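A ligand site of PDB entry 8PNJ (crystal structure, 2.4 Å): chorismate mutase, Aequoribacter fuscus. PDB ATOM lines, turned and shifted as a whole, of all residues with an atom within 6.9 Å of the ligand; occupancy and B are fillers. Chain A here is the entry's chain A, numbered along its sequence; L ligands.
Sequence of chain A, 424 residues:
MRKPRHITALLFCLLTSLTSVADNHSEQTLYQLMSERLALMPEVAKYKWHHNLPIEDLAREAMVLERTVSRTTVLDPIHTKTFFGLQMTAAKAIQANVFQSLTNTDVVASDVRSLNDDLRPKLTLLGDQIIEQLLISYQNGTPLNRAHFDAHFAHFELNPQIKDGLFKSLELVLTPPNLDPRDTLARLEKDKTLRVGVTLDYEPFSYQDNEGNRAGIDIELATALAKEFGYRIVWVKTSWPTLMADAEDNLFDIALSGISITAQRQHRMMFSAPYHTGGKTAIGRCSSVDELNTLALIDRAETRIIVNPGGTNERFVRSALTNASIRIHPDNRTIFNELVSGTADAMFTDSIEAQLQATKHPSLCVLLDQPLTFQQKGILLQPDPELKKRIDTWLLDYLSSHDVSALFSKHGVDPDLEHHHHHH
NH2 of Arg 37 lies within salt-bridge range of O4 of the ligand (2.4 Å). O1 of the ligand sits at hydrogen-bond distance from N of Asp 57 (2.5 Å). The backbone carbonyl oxygen (O) of Asp 57 lies within hydrogen-bond range of an oxygen (O1) of the ligand (3.4 Å). NZ of Lys 48 lies within salt-bridge range of O6 of the ligand, at 2.5 Å. The side-chain amide nitrogen (NE2) of Gln 95 is in hydrogen-bond range of an oxygen (O2) of the ligand, at 2.7 Å. O1 of the ligand sits at hydrogen-bond distance from OE2 of Glu 61, at 2.9 Å. O6 of the ligand is in salt-bridge range of NH2 of Arg 120 (3.1 Å). The backbone carbonyl oxygen of Ile 55 lies within hydrogen-bond range of an oxygen (O1) of the ligand (3.3 Å).
The side-chain carboxylate (OD2) of Asp 57 lies within salt-bridge range of the guanidinium group (NH2) of Arg 120 (2.9 Å). N of Arg 60 is in hydrogen-bond range of OD1 of Asp 57, at 3.3 Å. The side-chain amide oxygen (OE1) of Gln 95 is in hydrogen-bond range of the side-chain amino group (NZ) of Lys 48 (3.0 Å). NZ of Lys 48 is in hydrogen-bond range of O of Ile 55, at 2.8 Å. O of Ala 91 sits close to NE2 of Gln 95 (3.5 Å). SD of Met 41 lies within hydrogen-bond range of NE2 of Gln 95, 3.7 Å away. NH2 of Arg 60 sits close to O of Arg 120. The backbone NH of Arg 120 sits at hydrogen-bond distance from the backbone carbonyl oxygen of Leu 115 (2.7 Å).
Merely in contact with the ligand: Met 41, Val 44, Glu 56, Arg 60, Met 88, Ala 91 and Lys 92. Hydrophobic or aromatic side chains within 4 Å of the ligand: Met 41, Val 44, Met 88 and Ala 91. Of the 25 residues printed, 14 come within 4 Å of the ligand.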
ATOM      1  N   ARG A  37     -15.362 -26.542  13.154  1.00  0.00           N
ATOM      2  CA  ARG A  37     -15.763 -25.214  13.626  1.00  0.00           C
ATOM      3  C   ARG A  37     -16.451 -24.448  12.497  1.00  0.00           C
ATOM      4  O   ARG A  37     -17.534 -23.899  12.652  1.00  0.00           O
ATOM      5  CB  ARG A  37     -14.541 -24.456  14.163  1.00  0.00           C
ATOM      6  CG  ARG A  37     -14.850 -23.562  15.341  1.00  0.00           C
ATOM      7  CD  ARG A  37     -13.629 -22.986  16.044  1.00  0.00           C
ATOM      8  NE  ARG A  37     -13.451 -21.589  15.703  1.00  0.00           N
ATOM      9  CZ  ARG A  37     -14.321 -20.633  16.025  1.00  0.00           C
ATOM     10  NH1 ARG A  37     -14.892 -20.630  17.211  1.00  0.00           N
ATOM     11  NH2 ARG A  37     -14.611 -19.673  15.146  1.00  0.00           N
ATOM     12  N   MET A  41     -20.977 -23.169  10.858  1.00  0.00           N
ATOM     13  CA  MET A  41     -21.271 -21.772  10.563  1.00  0.00           C
ATOM     14  C   MET A  41     -22.452 -21.558   9.608  1.00  0.00           C
ATOM     15  O   MET A  41     -23.101 -20.524   9.700  1.00  0.00           O
ATOM     16  CB  MET A  41     -20.034 -21.070  10.000  1.00  0.00           C
ATOM     17  CG  MET A  41     -18.882 -21.033  11.004  1.00  0.00           C
ATOM     18  SD  MET A  41     -19.345 -20.332  12.630  1.00  0.00           S
ATOM     19  CE  MET A  41     -17.779 -20.516  13.461  1.00  0.00           C
ATOM     20  N   VAL A  44     -25.087 -21.351  12.090  1.00  0.00           N
ATOM     21  CA  VAL A  44     -25.061 -20.046  12.751  1.00  0.00           C
ATOM     22  C   VAL A  44     -25.726 -18.968  11.883  1.00  0.00           C
ATOM     23  O   VAL A  44     -26.363 -18.045  12.407  1.00  0.00           O
ATOM     24  CB  VAL A  44     -23.646 -19.655  13.149  1.00  0.00           C
ATOM     25  CG1 VAL A  44     -23.657 -18.347  13.910  1.00  0.00           C
ATOM     26  CG2 VAL A  44     -22.928 -20.744  13.959  1.00  0.00           C
ATOM     27  N   LYS A  48     -29.040 -16.484  12.369  1.00  0.00           N
ATOM     28  CA  LYS A  48     -28.867 -15.035  12.277  1.00  0.00           C
ATOM     29  C   LYS A  48     -29.725 -14.451  11.150  1.00  0.00           C
ATOM     30  O   LYS A  48     -30.217 -13.341  11.304  1.00  0.00           O
ATOM     31  CB  LYS A  48     -27.407 -14.653  12.038  1.00  0.00           C
ATOM     32  CG  LYS A  48     -26.581 -14.618  13.310  1.00  0.00           C
ATOM     33  CD  LYS A  48     -25.114 -14.522  13.058  1.00  0.00           C
ATOM     34  CE  LYS A  48     -24.306 -14.439  14.323  1.00  0.00           C
ATOM     35  NZ  LYS A  48     -22.885 -14.700  14.024  1.00  0.00           N
ATOM     36  N   PRO A  54     -26.927  -9.342  12.480  1.00  0.00           N
ATOM     37  CA  PRO A  54     -25.643  -9.218  11.797  1.00  0.00           C
ATOM     38  C   PRO A  54     -24.798 -10.491  11.969  1.00  0.00           C
ATOM     39  O   PRO A  54     -25.031 -11.307  12.867  1.00  0.00           O
ATOM     40  CB  PRO A  54     -24.982  -7.966  12.419  1.00  0.00           C
ATOM     41  CG  PRO A  54     -25.835  -7.576  13.659  1.00  0.00           C
ATOM     42  CD  PRO A  54     -27.101  -8.413  13.618  1.00  0.00           C
ATOM     43  N   ILE A  55     -23.812 -10.657  11.074  1.00  0.00           N
ATOM     44  CA  ILE A  55     -22.807 -11.709  11.142  1.00  0.00           C
ATOM     45  C   ILE A  55     -21.829 -11.447  12.305  1.00  0.00           C
ATOM     46  O   ILE A  55     -21.643 -12.287  13.190  1.00  0.00           O
ATOM     47  CB  ILE A  55     -22.113 -11.854   9.771  1.00  0.00           C
ATOM     48  CG1 ILE A  55     -23.135 -12.300   8.722  1.00  0.00           C
ATOM     49  CG2 ILE A  55     -20.917 -12.792   9.836  1.00  0.00           C
ATOM     50  CD1 ILE A  55     -22.556 -12.985   7.514  1.00  0.00           C
ATOM     51  N   GLU A  56     -21.204 -10.262  12.318  1.00  0.00           N
ATOM     52  CA  GLU A  56     -20.205  -9.980  13.331  1.00  0.00           C
ATOM     53  C   GLU A  56     -20.866  -9.729  14.686  1.00  0.00           C
ATOM     54  O   GLU A  56     -21.697  -8.843  14.835  1.00  0.00           O
ATOM     55  CB  GLU A  56     -19.309  -8.817  12.899  1.00  0.00           C
ATOM     56  CG  GLU A  56     -18.080  -8.634  13.770  1.00  0.00           C
ATOM     57  CD  GLU A  56     -17.108  -7.654  13.147  1.00  0.00           C
ATOM     58  OE1 GLU A  56     -17.354  -6.430  13.284  1.00  0.00           O
ATOM     59  OE2 GLU A  56     -16.145  -8.103  12.478  1.00  0.00           O
ATOM     60  N   ASP A  57     -20.470 -10.545  15.670  1.00  0.00           N
ATOM     61  CA  ASP A  57     -20.810 -10.303  17.069  1.00  0.00           C
ATOM     62  C   ASP A  57     -19.509 -10.118  17.850  1.00  0.00           C
ATOM     63  O   ASP A  57     -18.893 -11.102  18.233  1.00  0.00           O
ATOM     64  CB  ASP A  57     -21.703 -11.423  17.591  1.00  0.00           C
ATOM     65  CG  ASP A  57     -22.220 -11.189  18.991  1.00  0.00           C
ATOM     66  OD1 ASP A  57     -21.695 -10.265  19.680  1.00  0.00           O
ATOM     67  OD2 ASP A  57     -23.134 -11.943  19.400  1.00  0.00           O
ATOM     68  N   LEU A  58     -19.121  -8.846  18.069  1.00  0.00           N
ATOM     69  CA  LEU A  58     -17.812  -8.482  18.601  1.00  0.00           C
ATOM     70  C   LEU A  58     -17.664  -8.876  20.078  1.00  0.00           C
ATOM     71  O   LEU A  58     -16.578  -9.225  20.535  1.00  0.00           O
ATOM     72  CB  LEU A  58     -17.609  -6.970  18.465  1.00  0.00           C
ATOM     73  CG  LEU A  58     -17.267  -6.463  17.069  1.00  0.00           C
ATOM     74  CD1 LEU A  58     -17.236  -4.934  17.054  1.00  0.00           C
ATOM     75  CD2 LEU A  58     -15.951  -7.060  16.560  1.00  0.00           C
ATOM     76  N   ALA A  59     -18.747  -8.738  20.831  1.00  0.00           N
ATOM     77  CA  ALA A  59     -18.794  -9.160  22.228  1.00  0.00           C
ATOM     78  C   ALA A  59     -18.539 -10.668  22.362  1.00  0.00           C
ATOM     79  O   ALA A  59     -17.743 -11.087  23.205  1.00  0.00           O
ATOM     80  CB  ALA A  59     -20.143  -8.760  22.805  1.00  0.00           C
ATOM     81  N   ARG A  60     -19.230 -11.489  21.560  1.00  0.00           N
ATOM     82  CA  ARG A  60     -18.928 -12.900  21.500  1.00  0.00           C
ATOM     83  C   ARG A  60     -17.459 -13.126  21.132  1.00  0.00           C
ATOM     84  O   ARG A  60     -16.803 -13.970  21.750  1.00  0.00           O
ATOM     85  CB  ARG A  60     -19.824 -13.617  20.503  1.00  0.00           C
ATOM     86  CG  ARG A  60     -19.419 -15.060  20.224  1.00  0.00           C
ATOM     87  CD  ARG A  60     -19.526 -15.886  21.475  1.00  0.00           C
ATOM     88  NE  ARG A  60     -19.439 -17.311  21.219  1.00  0.00           N
ATOM     89  CZ  ARG A  60     -19.450 -18.230  22.176  1.00  0.00           C
ATOM     90  NH1 ARG A  60     -19.544 -17.845  23.446  1.00  0.00           N
ATOM     91  NH2 ARG A  60     -19.291 -19.507  21.871  1.00  0.00           N
ATOM     92  N   GLU A  61     -16.958 -12.412  20.116  1.00  0.00           N
ATOM     93  CA  GLU A  61     -15.574 -12.550  19.692  1.00  0.00           C
ATOM     94  C   GLU A  61     -14.603 -12.304  20.846  1.00  0.00           C
ATOM     95  O   GLU A  61     -13.658 -13.073  21.028  1.00  0.00           O
ATOM     96  CB  GLU A  61     -15.298 -11.633  18.490  1.00  0.00           C
ATOM     97  CG  GLU A  61     -15.860 -12.196  17.187  1.00  0.00           C
ATOM     98  CD  GLU A  61     -15.419 -11.511  15.903  1.00  0.00           C
ATOM     99  OE1 GLU A  61     -14.387 -10.791  15.896  1.00  0.00           O
ATOM    100  OE2 GLU A  61     -16.115 -11.712  14.896  1.00  0.00           O
ATOM    101  N   VAL A  64     -14.594 -15.117  23.368  1.00  0.00           N
ATOM    102  CA  VAL A  64     -13.869 -16.278  22.822  1.00  0.00           C
ATOM    103  C   VAL A  64     -12.359 -16.016  22.840  1.00  0.00           C
ATOM    104  O   VAL A  64     -11.570 -16.906  23.141  1.00  0.00           O
ATOM    105  CB  VAL A  64     -14.324 -16.693  21.405  1.00  0.00           C
ATOM    106  CG1 VAL A  64     -13.365 -17.696  20.753  1.00  0.00           C
ATOM    107  CG2 VAL A  64     -15.770 -17.228  21.376  1.00  0.00           C
ATOM    108  N   PHE A  84      -6.768 -17.400  16.175  1.00  0.00           N
ATOM    109  CA  PHE A  84      -8.178 -17.484  16.516  1.00  0.00           C
ATOM    110  C   PHE A  84      -8.998 -16.418  15.745  1.00  0.00           C
ATOM    111  O   PHE A  84     -10.073 -16.745  15.233  1.00  0.00           O
ATOM    112  CB  PHE A  84      -8.370 -17.551  18.040  1.00  0.00           C
ATOM    113  CG  PHE A  84      -8.338 -18.986  18.542  1.00  0.00           C
ATOM    114  CD1 PHE A  84      -7.146 -19.655  18.775  1.00  0.00           C
ATOM    115  CD2 PHE A  84      -9.520 -19.699  18.694  1.00  0.00           C
ATOM    116  CE1 PHE A  84      -7.135 -20.979  19.183  1.00  0.00           C
ATOM    117  CE2 PHE A  84      -9.505 -21.030  19.114  1.00  0.00           C
ATOM    118  CZ  PHE A  84      -8.314 -21.665  19.371  1.00  0.00           C
ATOM    119  N   GLY A  85      -8.493 -15.184  15.605  1.00  0.00           N
ATOM    120  CA  GLY A  85      -9.158 -14.135  14.849  1.00  0.00           C
ATOM    121  C   GLY A  85      -9.417 -14.482  13.379  1.00  0.00           C
ATOM    122  O   GLY A  85     -10.434 -14.075  12.801  1.00  0.00           O
ATOM    123  N   GLN A  87      -9.668 -17.671  12.156  1.00  0.00           N
ATOM    124  CA  GLN A  87     -10.764 -18.636  12.208  1.00  0.00           C
ATOM    125  C   GLN A  87     -12.128 -17.930  12.312  1.00  0.00           C
ATOM    126  O   GLN A  87     -13.108 -18.421  11.749  1.00  0.00           O
ATOM    127  CB  GLN A  87     -10.607 -19.614  13.368  1.00  0.00           C
ATOM    128  CG  GLN A  87      -9.375 -20.494  13.207  1.00  0.00           C
ATOM    129  CD  GLN A  87      -9.241 -21.379  14.411  1.00  0.00           C
ATOM    130  OE1 GLN A  87      -8.513 -21.042  15.353  1.00  0.00           O
ATOM    131  NE2 GLN A  87     -10.021 -22.456  14.393  1.00  0.00           N
ATOM    132  N   MET A  88     -12.181 -16.799  13.008  1.00  0.00           N
ATOM    133  CA  MET A  88     -13.432 -16.062  13.155  1.00  0.00           C
ATOM    134  C   MET A  88     -13.776 -15.353  11.845  1.00  0.00           C
ATOM    135  O   MET A  88     -14.908 -15.392  11.415  1.00  0.00           O
ATOM    136  CB  MET A  88     -13.359 -15.096  14.345  1.00  0.00           C
ATOM    137  CG  MET A  88     -13.457 -15.862  15.696  1.00  0.00           C
ATOM    138  SD  MET A  88     -13.188 -14.909  17.245  1.00  0.00           S
ATOM    139  CE  MET A  88     -12.552 -13.380  16.557  1.00  0.00           C
ATOM    140  N   THR A  89     -12.757 -14.794  11.184  1.00  0.00           N
ATOM    141  CA  THR A  89     -12.836 -14.207   9.856  1.00  0.00           C
ATOM    142  C   THR A  89     -13.249 -15.267   8.830  1.00  0.00           C
ATOM    143  O   THR A  89     -14.120 -15.018   8.014  1.00  0.00           O
ATOM    144  CB  THR A  89     -11.515 -13.508   9.514  1.00  0.00           C
ATOM    145  OG1 THR A  89     -11.341 -12.472  10.459  1.00  0.00           O
ATOM    146  CG2 THR A  89     -11.460 -12.900   8.128  1.00  0.00           C
ATOM    147  N   ALA A  90     -12.627 -16.449   8.863  1.00  0.00           N
ATOM    148  CA  ALA A  90     -13.095 -17.570   8.039  1.00  0.00           C
ATOM    149  C   ALA A  90     -14.550 -17.914   8.355  1.00  0.00           C
ATOM    150  O   ALA A  90     -15.353 -18.092   7.438  1.00  0.00           O
ATOM    151  CB  ALA A  90     -12.191 -18.756   8.193  1.00  0.00           C
ATOM    152  N   ALA A  91     -14.925 -17.902   9.650  1.00  0.00           N
ATOM    153  CA  ALA A  91     -16.292 -18.235  10.037  1.00  0.00           C
ATOM    154  C   ALA A  91     -17.314 -17.234   9.463  1.00  0.00           C
ATOM    155  O   ALA A  91     -18.325 -17.659   8.893  1.00  0.00           O
ATOM    156  CB  ALA A  91     -16.384 -18.381  11.531  1.00  0.00           C
ATOM    157  N   LYS A  92     -17.043 -15.918   9.578  1.00  0.00           N
ATOM    158  CA  LYS A  92     -17.886 -14.868   8.996  1.00  0.00           C
ATOM    159  C   LYS A  92     -17.979 -14.897   7.461  1.00  0.00           C
ATOM    160  O   LYS A  92     -19.044 -14.651   6.918  1.00  0.00           O
ATOM    161  CB  LYS A  92     -17.403 -13.498   9.467  1.00  0.00           C
ATOM    162  CG  LYS A  92     -17.637 -13.287  10.956  1.00  0.00           C
ATOM    163  CD  LYS A  92     -16.479 -12.768  11.734  1.00  0.00           C
ATOM    164  CE  LYS A  92     -16.107 -11.330  11.429  1.00  0.00           C
ATOM    165  NZ  LYS A  92     -15.381 -10.759  12.577  1.00  0.00           N
ATOM    166  N   GLN A  95     -20.291 -17.476   6.693  1.00  0.00           N
ATOM    167  CA  GLN A  95     -21.648 -17.110   7.082  1.00  0.00           C
ATOM    168  C   GLN A  95     -22.248 -16.186   6.001  1.00  0.00           C
ATOM    169  O   GLN A  95     -23.438 -16.276   5.738  1.00  0.00           O
ATOM    170  CB  GLN A  95     -21.679 -16.471   8.482  1.00  0.00           C
ATOM    171  CG  GLN A  95     -21.578 -17.463   9.639  1.00  0.00           C
ATOM    172  CD  GLN A  95     -21.457 -16.740  10.966  1.00  0.00           C
ATOM    173  OE1 GLN A  95     -22.394 -16.068  11.401  1.00  0.00           O
ATOM    174  NE2 GLN A  95     -20.305 -16.889  11.621  1.00  0.00           N
ATOM    175  N   LEU A 115     -28.549 -20.714  18.512  1.00  0.00           N
ATOM    176  CA  LEU A 115     -27.209 -20.172  18.638  1.00  0.00           C
ATOM    177  C   LEU A 115     -26.640 -20.393  20.052  1.00  0.00           C
ATOM    178  O   LEU A 115     -25.517 -20.877  20.177  1.00  0.00           O
ATOM    179  CB  LEU A 115     -27.262 -18.680  18.278  1.00  0.00           C
ATOM    180  CG  LEU A 115     -25.891 -18.022  18.122  1.00  0.00           C
ATOM    181  CD1 LEU A 115     -25.233 -18.483  16.836  1.00  0.00           C
ATOM    182  CD2 LEU A 115     -25.980 -16.504  18.178  1.00  0.00           C
ATOM    183  N   ARG A 120     -23.231 -22.354  19.899  1.00  0.00           N
ATOM    184  CA  ARG A 120     -22.073 -21.745  20.563  1.00  0.00           C
ATOM    185  C   ARG A 120     -21.446 -22.691  21.603  1.00  0.00           C
ATOM    186  O   ARG A 120     -20.228 -22.738  21.711  1.00  0.00           O
ATOM    187  CB  ARG A 120     -22.434 -20.386  21.167  1.00  0.00           C
ATOM    188  CG  ARG A 120     -22.365 -19.255  20.164  1.00  0.00           C
ATOM    189  CD  ARG A 120     -22.977 -17.955  20.631  1.00  0.00           C
ATOM    190  NE  ARG A 120     -22.642 -16.815  19.779  1.00  0.00           N
ATOM    191  CZ  ARG A 120     -23.233 -15.614  19.882  1.00  0.00           C
ATOM    192  NH1 ARG A 120     -23.865 -15.283  21.002  1.00  0.00           N
ATOM    193  NH2 ARG A 120     -23.208 -14.780  18.854  1.00  0.00           N
ATOM    194  N   LEU A 123     -19.185 -24.690  19.553  1.00  0.00           N
ATOM    195  CA  LEU A 123     -18.010 -23.919  19.161  1.00  0.00           C
ATOM    196  C   LEU A 123     -17.038 -23.738  20.341  1.00  0.00           C
ATOM    197  O   LEU A 123     -15.814 -23.778  20.162  1.00  0.00           O
ATOM    198  CB  LEU A 123     -18.430 -22.541  18.624  1.00  0.00           C
ATOM    199  CG  LEU A 123     -19.282 -22.541  17.349  1.00  0.00           C
ATOM    200  CD1 LEU A 123     -19.622 -21.109  16.941  1.00  0.00           C
ATOM    201  CD2 LEU A 123     -18.593 -23.283  16.212  1.00  0.00           C
HETATM  202  C1  LIG L   1     -17.806 -16.343  15.546  1.00  0.00           C
HETATM  203  C2  LIG L   1     -18.072 -15.460  16.758  1.00  0.00           C
HETATM  204  C3  LIG L   1     -18.748 -14.316  16.678  1.00  0.00           C
HETATM  205  C4  LIG L   1     -19.389 -13.828  15.414  1.00  0.00           C
HETATM  206  O1  LIG L   1     -18.941 -12.487  15.144  1.00  0.00           O
HETATM  207  C5  LIG L   1     -19.106 -14.738  14.216  1.00  0.00           C
HETATM  208  C6  LIG L   1     -17.749 -15.438  14.293  1.00  0.00           C
HETATM  209  O2  LIG L   1     -20.201 -15.666  14.037  1.00  0.00           O
HETATM  210  C7  LIG L   1     -20.264 -16.784  14.951  1.00  0.00           C
HETATM  211  C8  LIG L   1     -18.886 -17.391  15.210  1.00  0.00           C
HETATM  212  C9  LIG L   1     -16.582 -17.185  15.908  1.00  0.00           C
HETATM  213  O3  LIG L   1     -16.452 -17.527  17.098  1.00  0.00           O
HETATM  214  O4  LIG L   1     -15.803 -17.565  15.030  1.00  0.00           O
HETATM  215  C10 LIG L   1     -21.027 -16.434  16.244  1.00  0.00           C
HETATM  216  O5  LIG L   1     -20.748 -17.001  17.309  1.00  0.00           O
HETATM  217  O6  LIG L   1     -21.953 -15.614  16.189  1.00  0.00           O
